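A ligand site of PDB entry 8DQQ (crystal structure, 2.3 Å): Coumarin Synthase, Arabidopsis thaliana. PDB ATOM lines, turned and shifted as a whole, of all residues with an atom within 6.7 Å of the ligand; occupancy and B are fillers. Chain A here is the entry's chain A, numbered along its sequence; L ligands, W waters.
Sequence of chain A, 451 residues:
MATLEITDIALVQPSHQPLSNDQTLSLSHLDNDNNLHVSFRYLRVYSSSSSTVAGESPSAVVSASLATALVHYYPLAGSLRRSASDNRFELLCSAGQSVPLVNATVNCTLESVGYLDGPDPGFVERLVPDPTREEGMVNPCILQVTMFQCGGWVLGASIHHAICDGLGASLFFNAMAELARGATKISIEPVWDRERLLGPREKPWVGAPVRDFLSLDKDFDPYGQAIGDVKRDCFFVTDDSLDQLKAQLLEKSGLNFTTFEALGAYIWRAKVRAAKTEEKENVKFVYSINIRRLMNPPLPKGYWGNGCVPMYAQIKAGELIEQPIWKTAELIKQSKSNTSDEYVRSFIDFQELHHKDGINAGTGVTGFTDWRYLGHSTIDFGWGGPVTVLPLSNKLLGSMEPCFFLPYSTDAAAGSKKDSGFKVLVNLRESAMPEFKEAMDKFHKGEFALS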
ATOM      1  N   PHE A  40      10.387  13.472  17.113  1.00  0.00           N
ATOM      2  CA  PHE A  40      10.413  13.681  18.556  1.00  0.00           C
ATOM      3  C   PHE A  40       9.457  14.815  18.932  1.00  0.00           C
ATOM      4  O   PHE A  40       9.532  15.905  18.358  1.00  0.00           O
ATOM      5  CB  PHE A  40      11.822  13.984  19.052  1.00  0.00           C
ATOM      6  CG  PHE A  40      11.914  14.098  20.540  1.00  0.00           C
ATOM      7  CD1 PHE A  40      11.846  12.960  21.336  1.00  0.00           C
ATOM      8  CD2 PHE A  40      12.033  15.331  21.160  1.00  0.00           C
ATOM      9  CE1 PHE A  40      11.920  13.050  22.707  1.00  0.00           C
ATOM     10  CE2 PHE A  40      12.110  15.431  22.531  1.00  0.00           C
ATOM     11  CZ  PHE A  40      12.044  14.282  23.308  1.00  0.00           C
ATOM     12  N   TYR A  42       7.809  17.126  22.049  1.00  0.00           N
ATOM     13  CA  TYR A  42       7.849  17.606  23.415  1.00  0.00           C
ATOM     14  C   TYR A  42       7.261  19.005  23.455  1.00  0.00           C
ATOM     15  O   TYR A  42       7.118  19.667  22.429  1.00  0.00           O
ATOM     16  CB  TYR A  42       9.269  17.598  24.008  1.00  0.00           C
ATOM     17  CG  TYR A  42      10.265  18.558  23.385  1.00  0.00           C
ATOM     18  CD1 TYR A  42      10.370  18.705  22.004  1.00  0.00           C
ATOM     19  CD2 TYR A  42      11.105  19.314  24.177  1.00  0.00           C
ATOM     20  CE1 TYR A  42      11.277  19.577  21.437  1.00  0.00           C
ATOM     21  CE2 TYR A  42      12.019  20.193  23.632  1.00  0.00           C
ATOM     22  CZ  TYR A  42      12.103  20.315  22.257  1.00  0.00           C
ATOM     23  OH  TYR A  42      13.017  21.195  21.712  1.00  0.00           O
ATOM     24  N   ARG A  44       6.732  22.771  26.011  1.00  0.00           N
ATOM     25  CA  ARG A  44       7.126  23.655  27.101  1.00  0.00           C
ATOM     26  C   ARG A  44       5.917  24.449  27.547  1.00  0.00           C
ATOM     27  O   ARG A  44       5.155  24.952  26.710  1.00  0.00           O
ATOM     28  CB  ARG A  44       8.251  24.591  26.680  1.00  0.00           C
ATOM     29  CG  ARG A  44       9.495  23.880  26.207  1.00  0.00           C
ATOM     30  CD  ARG A  44       9.688  24.063  24.711  1.00  0.00           C
ATOM     31  NE  ARG A  44      10.955  23.513  24.264  1.00  0.00           N
ATOM     32  CZ  ARG A  44      12.130  24.097  24.450  1.00  0.00           C
ATOM     33  NH1 ARG A  44      12.230  25.241  25.113  1.00  0.00           N
ATOM     34  NH2 ARG A  44      13.226  23.529  23.970  1.00  0.00           N
ATOM     35  N   SER A 158       7.269  19.192  17.122  1.00  0.00           N
ATOM     36  CA  SER A 158       7.552  17.890  16.540  1.00  0.00           C
ATOM     37  C   SER A 158       8.685  18.076  15.540  1.00  0.00           C
ATOM     38  O   SER A 158       8.504  18.710  14.496  1.00  0.00           O
ATOM     39  CB  SER A 158       6.315  17.304  15.881  1.00  0.00           C
ATOM     40  OG  SER A 158       6.644  16.671  14.653  1.00  0.00           O
ATOM     41  N   ILE A 159       9.869  17.551  15.868  1.00  0.00           N
ATOM     42  CA  ILE A 159      11.039  17.680  15.016  1.00  0.00           C
ATOM     43  C   ILE A 159      11.532  16.286  14.662  1.00  0.00           C
ATOM     44  O   ILE A 159      11.664  15.419  15.533  1.00  0.00           O
ATOM     45  CB  ILE A 159      12.148  18.508  15.677  1.00  0.00           C
ATOM     46  CG1 ILE A 159      11.630  19.900  16.036  1.00  0.00           C
ATOM     47  CG2 ILE A 159      13.353  18.617  14.753  1.00  0.00           C
ATOM     48  CD1 ILE A 159      12.724  20.896  16.369  1.00  0.00           C
ATOM     49  N   HIS A 160      11.821  16.077  13.374  1.00  0.00           N
ATOM     50  CA  HIS A 160      12.430  14.825  12.936  1.00  0.00           C
ATOM     51  C   HIS A 160      13.855  14.765  13.450  1.00  0.00           C
ATOM     52  O   HIS A 160      14.640  15.702  13.271  1.00  0.00           O
ATOM     53  CB  HIS A 160      12.390  14.737  11.408  1.00  0.00           C
ATOM     54  CG  HIS A 160      12.665  13.364  10.891  1.00  0.00           C
ATOM     55  ND1 HIS A 160      13.939  12.848  10.764  1.00  0.00           N
ATOM     56  CD2 HIS A 160      11.828  12.391  10.447  1.00  0.00           C
ATOM     57  CE1 HIS A 160      13.883  11.623  10.274  1.00  0.00           C
ATOM     58  NE2 HIS A 160      12.610  11.324  10.073  1.00  0.00           N
ATOM     59  N   HIS A 161      14.197  13.644  14.094  1.00  0.00           N
ATOM     60  CA  HIS A 161      15.455  13.561  14.825  1.00  0.00           C
ATOM     61  C   HIS A 161      16.672  13.582  13.911  1.00  0.00           C
ATOM     62  O   HIS A 161      17.772  13.911  14.375  1.00  0.00           O
ATOM     63  CB  HIS A 161      15.466  12.292  15.692  1.00  0.00           C
ATOM     64  CG  HIS A 161      16.323  12.404  16.905  1.00  0.00           C
ATOM     65  ND1 HIS A 161      17.532  13.064  16.909  1.00  0.00           N
ATOM     66  CD2 HIS A 161      16.153  11.923  18.168  1.00  0.00           C
ATOM     67  CE1 HIS A 161      18.068  12.996  18.122  1.00  0.00           C
ATOM     68  NE2 HIS A 161      17.250  12.312  18.897  1.00  0.00           N
ATOM     69  N   ALA A 162      16.508  13.257  12.625  1.00  0.00           N
ATOM     70  CA  ALA A 162      17.634  13.286  11.697  1.00  0.00           C
ATOM     71  C   ALA A 162      18.194  14.685  11.500  1.00  0.00           C
ATOM     72  O   ALA A 162      19.358  14.819  11.093  1.00  0.00           O
ATOM     73  CB  ALA A 162      17.223  12.695  10.355  1.00  0.00           C
ATOM     74  N   ILE A 163      17.414  15.721  11.794  1.00  0.00           N
ATOM     75  CA  ILE A 163      17.879  17.079  11.501  1.00  0.00           C
ATOM     76  C   ILE A 163      18.705  17.643  12.655  1.00  0.00           C
ATOM     77  O   ILE A 163      19.685  18.360  12.418  1.00  0.00           O
ATOM     78  CB  ILE A 163      16.663  17.962  11.162  1.00  0.00           C
ATOM     79  CG1 ILE A 163      16.350  17.836   9.668  1.00  0.00           C
ATOM     80  CG2 ILE A 163      16.890  19.427  11.557  1.00  0.00           C
ATOM     81  CD1 ILE A 163      15.104  18.573   9.227  1.00  0.00           C
ATOM     82  N   CYS A 164      18.354  17.326  13.900  1.00  0.00           N
ATOM     83  CA  CYS A 164      19.083  17.880  15.039  1.00  0.00           C
ATOM     84  C   CYS A 164      18.857  16.987  16.253  1.00  0.00           C
ATOM     85  O   CYS A 164      17.944  16.147  16.267  1.00  0.00           O
ATOM     86  CB  CYS A 164      18.650  19.319  15.344  1.00  0.00           C
ATOM     87  SG  CYS A 164      16.883  19.507  15.716  1.00  0.00           S
ATOM     88  N   ASP A 165      19.689  17.184  17.267  1.00  0.00           N
ATOM     89  CA  ASP A 165      19.555  16.491  18.544  1.00  0.00           C
ATOM     90  C   ASP A 165      19.008  17.461  19.587  1.00  0.00           C
ATOM     91  O   ASP A 165      18.521  18.549  19.260  1.00  0.00           O
ATOM     92  CB  ASP A 165      20.906  15.889  18.962  1.00  0.00           C
ATOM     93  CG  ASP A 165      22.022  16.914  19.061  1.00  0.00           C
ATOM     94  OD1 ASP A 165      21.738  18.117  19.225  1.00  0.00           O
ATOM     95  OD2 ASP A 165      23.201  16.512  18.974  1.00  0.00           O
ATOM     96  N   GLY A 166      19.104  17.061  20.852  1.00  0.00           N
ATOM     97  CA  GLY A 166      18.619  17.873  21.954  1.00  0.00           C
ATOM     98  C   GLY A 166      19.271  19.237  22.043  1.00  0.00           C
ATOM     99  O   GLY A 166      18.597  20.266  21.960  1.00  0.00           O
ATOM    100  N   LEU A 167      20.599  19.267  22.204  1.00  0.00           N
ATOM    101  CA  LEU A 167      21.333  20.521  22.259  1.00  0.00           C
ATOM    102  C   LEU A 167      21.255  21.304  20.952  1.00  0.00           C
ATOM    103  O   LEU A 167      21.576  22.504  20.944  1.00  0.00           O
ATOM    104  CB  LEU A 167      22.789  20.253  22.620  1.00  0.00           C
ATOM    105  CG  LEU A 167      23.046  19.747  24.039  1.00  0.00           C
ATOM    106  CD1 LEU A 167      24.132  18.691  24.024  1.00  0.00           C
ATOM    107  CD2 LEU A 167      23.432  20.889  24.953  1.00  0.00           C
ATOM    108  N   GLY A 168      20.832  20.681  19.847  1.00  0.00           N
ATOM    109  CA  GLY A 168      20.690  21.379  18.590  1.00  0.00           C
ATOM    110  C   GLY A 168      19.388  22.139  18.485  1.00  0.00           C
ATOM    111  O   GLY A 168      19.349  23.275  17.983  1.00  0.00           O
ATOM    112  N   ALA A 169      18.293  21.520  18.934  1.00  0.00           N
ATOM    113  CA  ALA A 169      17.046  22.247  19.094  1.00  0.00           C
ATOM    114  C   ALA A 169      17.099  23.241  20.242  1.00  0.00           C
ATOM    115  O   ALA A 169      16.175  24.042  20.390  1.00  0.00           O
ATOM    116  CB  ALA A 169      15.894  21.271  19.293  1.00  0.00           C
ATOM    117  N   SER A 170      18.150  23.202  21.061  1.00  0.00           N
ATOM    118  CA  SER A 170      18.349  24.213  22.101  1.00  0.00           C
ATOM    119  C   SER A 170      18.934  25.484  21.515  1.00  0.00           C
ATOM    120  O   SER A 170      18.488  26.591  21.829  1.00  0.00           O
ATOM    121  CB  SER A 170      19.243  23.653  23.214  1.00  0.00           C
ATOM    122  OG  SER A 170      19.020  24.335  24.435  1.00  0.00           O
ATOM    123  N   PHE A 173      16.188  27.217  19.533  1.00  0.00           N
ATOM    124  CA  PHE A 173      15.160  27.862  20.358  1.00  0.00           C
ATOM    125  C   PHE A 173      15.746  28.983  21.202  1.00  0.00           C
ATOM    126  O   PHE A 173      15.073  30.006  21.411  1.00  0.00           O
ATOM    127  CB  PHE A 173      14.470  26.830  21.242  1.00  0.00           C
ATOM    128  CG  PHE A 173      13.452  25.994  20.523  1.00  0.00           C
ATOM    129  CD1 PHE A 173      12.801  26.477  19.386  1.00  0.00           C
ATOM    130  CD2 PHE A 173      13.125  24.726  20.969  1.00  0.00           C
ATOM    131  CE1 PHE A 173      11.865  25.708  18.725  1.00  0.00           C
ATOM    132  CE2 PHE A 173      12.186  23.948  20.309  1.00  0.00           C
ATOM    133  CZ  PHE A 173      11.557  24.444  19.187  1.00  0.00           C
ATOM    134  N   SER A 288      22.215   8.587  25.404  1.00  0.00           N
ATOM    135  CA  SER A 288      23.040   9.396  24.519  1.00  0.00           C
ATOM    136  C   SER A 288      23.891  10.368  25.330  1.00  0.00           C
ATOM    137  O   SER A 288      23.459  10.859  26.374  1.00  0.00           O
ATOM    138  CB  SER A 288      22.180  10.164  23.525  1.00  0.00           C
ATOM    139  OG  SER A 288      22.621   9.949  22.194  1.00  0.00           O
ATOM    140  N   ASN A 306      22.971  16.476  14.895  1.00  0.00           N
ATOM    141  CA  ASN A 306      23.127  15.410  15.869  1.00  0.00           C
ATOM    142  C   ASN A 306      24.604  15.252  16.207  1.00  0.00           C
ATOM    143  O   ASN A 306      25.405  14.849  15.347  1.00  0.00           O
ATOM    144  CB  ASN A 306      22.535  14.108  15.336  1.00  0.00           C
ATOM    145  CG  ASN A 306      21.013  14.117  15.329  1.00  0.00           C
ATOM    146  OD1 ASN A 306      20.386  13.862  16.352  1.00  0.00           O
ATOM    147  ND2 ASN A 306      20.424  14.411  14.179  1.00  0.00           N
ATOM    148  N   THR A 369      16.848   8.854  29.143  1.00  0.00           N
ATOM    149  CA  THR A 369      17.208  10.235  28.864  1.00  0.00           C
ATOM    150  C   THR A 369      17.075  11.066  30.129  1.00  0.00           C
ATOM    151  O   THR A 369      16.078  10.946  30.849  1.00  0.00           O
ATOM    152  CB  THR A 369      16.341  10.829  27.734  1.00  0.00           C
ATOM    153  OG1 THR A 369      16.415   9.983  26.579  1.00  0.00           O
ATOM    154  CG2 THR A 369      16.837  12.209  27.356  1.00  0.00           C
ATOM    155  N   TRP A 371      16.973  14.721  31.676  1.00  0.00           N
ATOM    156  CA  TRP A 371      16.672  16.107  31.346  1.00  0.00           C
ATOM    157  C   TRP A 371      16.808  17.052  32.530  1.00  0.00           C
ATOM    158  O   TRP A 371      16.462  18.239  32.398  1.00  0.00           O
ATOM    159  CB  TRP A 371      15.253  16.208  30.779  1.00  0.00           C
ATOM    160  CG  TRP A 371      15.162  15.947  29.311  1.00  0.00           C
ATOM    161  CD1 TRP A 371      16.086  15.324  28.530  1.00  0.00           C
ATOM    162  CD2 TRP A 371      14.080  16.312  28.441  1.00  0.00           C
ATOM    163  NE1 TRP A 371      15.650  15.288  27.226  1.00  0.00           N
ATOM    164  CE2 TRP A 371      14.430  15.884  27.143  1.00  0.00           C
ATOM    165  CE3 TRP A 371      12.865  16.966  28.636  1.00  0.00           C
ATOM    166  CZ2 TRP A 371      13.587  16.081  26.047  1.00  0.00           C
ATOM    167  CZ3 TRP A 371      12.030  17.160  27.543  1.00  0.00           C
ATOM    168  CH2 TRP A 371      12.403  16.713  26.262  1.00  0.00           C
ATOM    169  N   LEU A 396      12.590   6.033  20.691  1.00  0.00           N
ATOM    170  CA  LEU A 396      13.810   6.779  20.982  1.00  0.00           C
ATOM    171  C   LEU A 396      14.947   5.807  21.265  1.00  0.00           C
ATOM    172  O   LEU A 396      14.771   4.842  22.031  1.00  0.00           O
ATOM    173  CB  LEU A 396      13.593   7.702  22.188  1.00  0.00           C
ATOM    174  CG  LEU A 396      14.231   9.091  22.282  1.00  0.00           C
ATOM    175  CD1 LEU A 396      14.357   9.489  23.749  1.00  0.00           C
ATOM    176  CD2 LEU A 396      15.571   9.174  21.582  1.00  0.00           C
ATOM    177  N   LEU A 397      16.124   6.045  20.668  1.00  0.00           N
ATOM    178  CA  LEU A 397      17.335   5.280  20.967  1.00  0.00           C
ATOM    179  C   LEU A 397      17.159   3.796  20.680  1.00  0.00           C
ATOM    180  O   LEU A 397      17.675   2.944  21.403  1.00  0.00           O
ATOM    181  CB  LEU A 397      17.776   5.491  22.416  1.00  0.00           C
ATOM    182  CG  LEU A 397      18.260   6.884  22.821  1.00  0.00           C
ATOM    183  CD1 LEU A 397      17.814   7.215  24.225  1.00  0.00           C
ATOM    184  CD2 LEU A 397      19.776   6.962  22.717  1.00  0.00           C
ATOM    185  N   PHE A 404      12.402   8.825  30.887  1.00  0.00           N
ATOM    186  CA  PHE A 404      12.948  10.170  31.021  1.00  0.00           C
ATOM    187  C   PHE A 404      13.067  10.549  32.488  1.00  0.00           C
ATOM    188  O   PHE A 404      12.190  10.241  33.293  1.00  0.00           O
ATOM    189  CB  PHE A 404      12.062  11.205  30.312  1.00  0.00           C
ATOM    190  CG  PHE A 404      11.994  11.031  28.824  1.00  0.00           C
ATOM    191  CD1 PHE A 404      11.022  10.231  28.250  1.00  0.00           C
ATOM    192  CD2 PHE A 404      12.899  11.667  27.993  1.00  0.00           C
ATOM    193  CE1 PHE A 404      10.957  10.065  26.876  1.00  0.00           C
ATOM    194  CE2 PHE A 404      12.834  11.501  26.619  1.00  0.00           C
ATOM    195  CZ  PHE A 404      11.857  10.701  26.064  1.00  0.00           C
HETATM  196  O1  LIG L   1      16.581  12.993  22.592  1.00  0.00           O
HETATM  197  C1  LIG L   1      16.185  14.103  22.318  1.00  0.00           C
HETATM  198  C2  LIG L   1      15.901  15.125  23.302  1.00  0.00           C
HETATM  199  C3  LIG L   1      15.453  16.371  22.830  1.00  0.00           C
HETATM  200  C4  LIG L   1      15.277  16.599  21.420  1.00  0.00           C
HETATM  201  O2  LIG L   1      16.002  14.364  20.967  1.00  0.00           O
HETATM  202  C5  LIG L   1      15.570  15.573  20.511  1.00  0.00           C
HETATM  203  C6  LIG L   1      15.412  15.753  19.099  1.00  0.00           C
HETATM  204  C7  LIG L   1      14.960  16.980  18.616  1.00  0.00           C
HETATM  205  O3  LIG L   1      14.793  17.215  17.260  1.00  0.00           O
HETATM  206  C8  LIG L   1      14.669  18.027  19.504  1.00  0.00           C
HETATM  207  C9  LIG L   1      14.835  17.834  20.877  1.00  0.00           C
HETATM  208  O   HOH W   1      19.614  14.734  22.494  1.00  0.00           O
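Water W1 lies within hydrogen-bond range of the backbone NH of Gly 166 (2.9 Å) and an oxygen (O1) of the ligand (3.5 Å).
A ring nitrogen (ND1) of His 161 lies within hydrogen-bond range of the backbone carbonyl oxygen (O) of Cys 164 (3.2 Å). The side-chain amide nitrogen of Asn 306 is in hydrogen-bond range of the backbone carbonyl oxygen of His 161. The backbone NH (N) of Phe 40 is in hydrogen-bond range of the backbone carbonyl oxygen (O) of Ile 159. OD1 of Asn 306 lies close to O of Cys 164 (3.3 Å). OD1 of Asp 165 lies within hydrogen-bond range of N of Leu 167, 3.4 Å away. The backbone NH (N) of Gly 168 is in hydrogen-bond range of the side-chain carboxylate (OD1) of Asp 165, 2.8 Å away. The side-chain hydroxyl of Tyr 42 lies within hydrogen-bond range of the guanidinium group of Arg 44 (3.3 Å).
Phe 40 touches the ligand (CE2 to C3, 3.5 Å). Tyr 42 touches the ligand (OH to C9, 3.9 Å). Ile 159 touches the ligand (CG2 to O3, 3.2 Å). Asp 165 touches the ligand (O to C8, 3.9 Å). Gly 166 touches the ligand. Ala 169 touches the ligand (CB to C8, 3.5 Å). Trp 371 touches the ligand (CZ2 to C2, 3.7 Å). Hydrophobic or aromatic side chains within 4 Å of the ligand: Phe 40, Tyr 42, Ile 159, His 161, Ala 169 and Trp 371. Nine residues have an atom within 4 Å of the ligand: Phe 40, Tyr 42, Ile 159, His 161, Cys 164, Asp 165, Gly 166, Ala 169 and Trp 371.
An oxygen (O2) of the ligand sits at hydrogen-bond distance from a ring nitrogen (NE2) of His 161 (3.2 Å). The backbone carbonyl oxygen (O) of Cys 164 lies within hydrogen-bond range of an oxygen (O3) of the ligand (3.5 Å). An oxygen (O3) of the ligand is in hydrogen-bond range of the side-chain sulfur of Cys 164 (3.5 Å).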
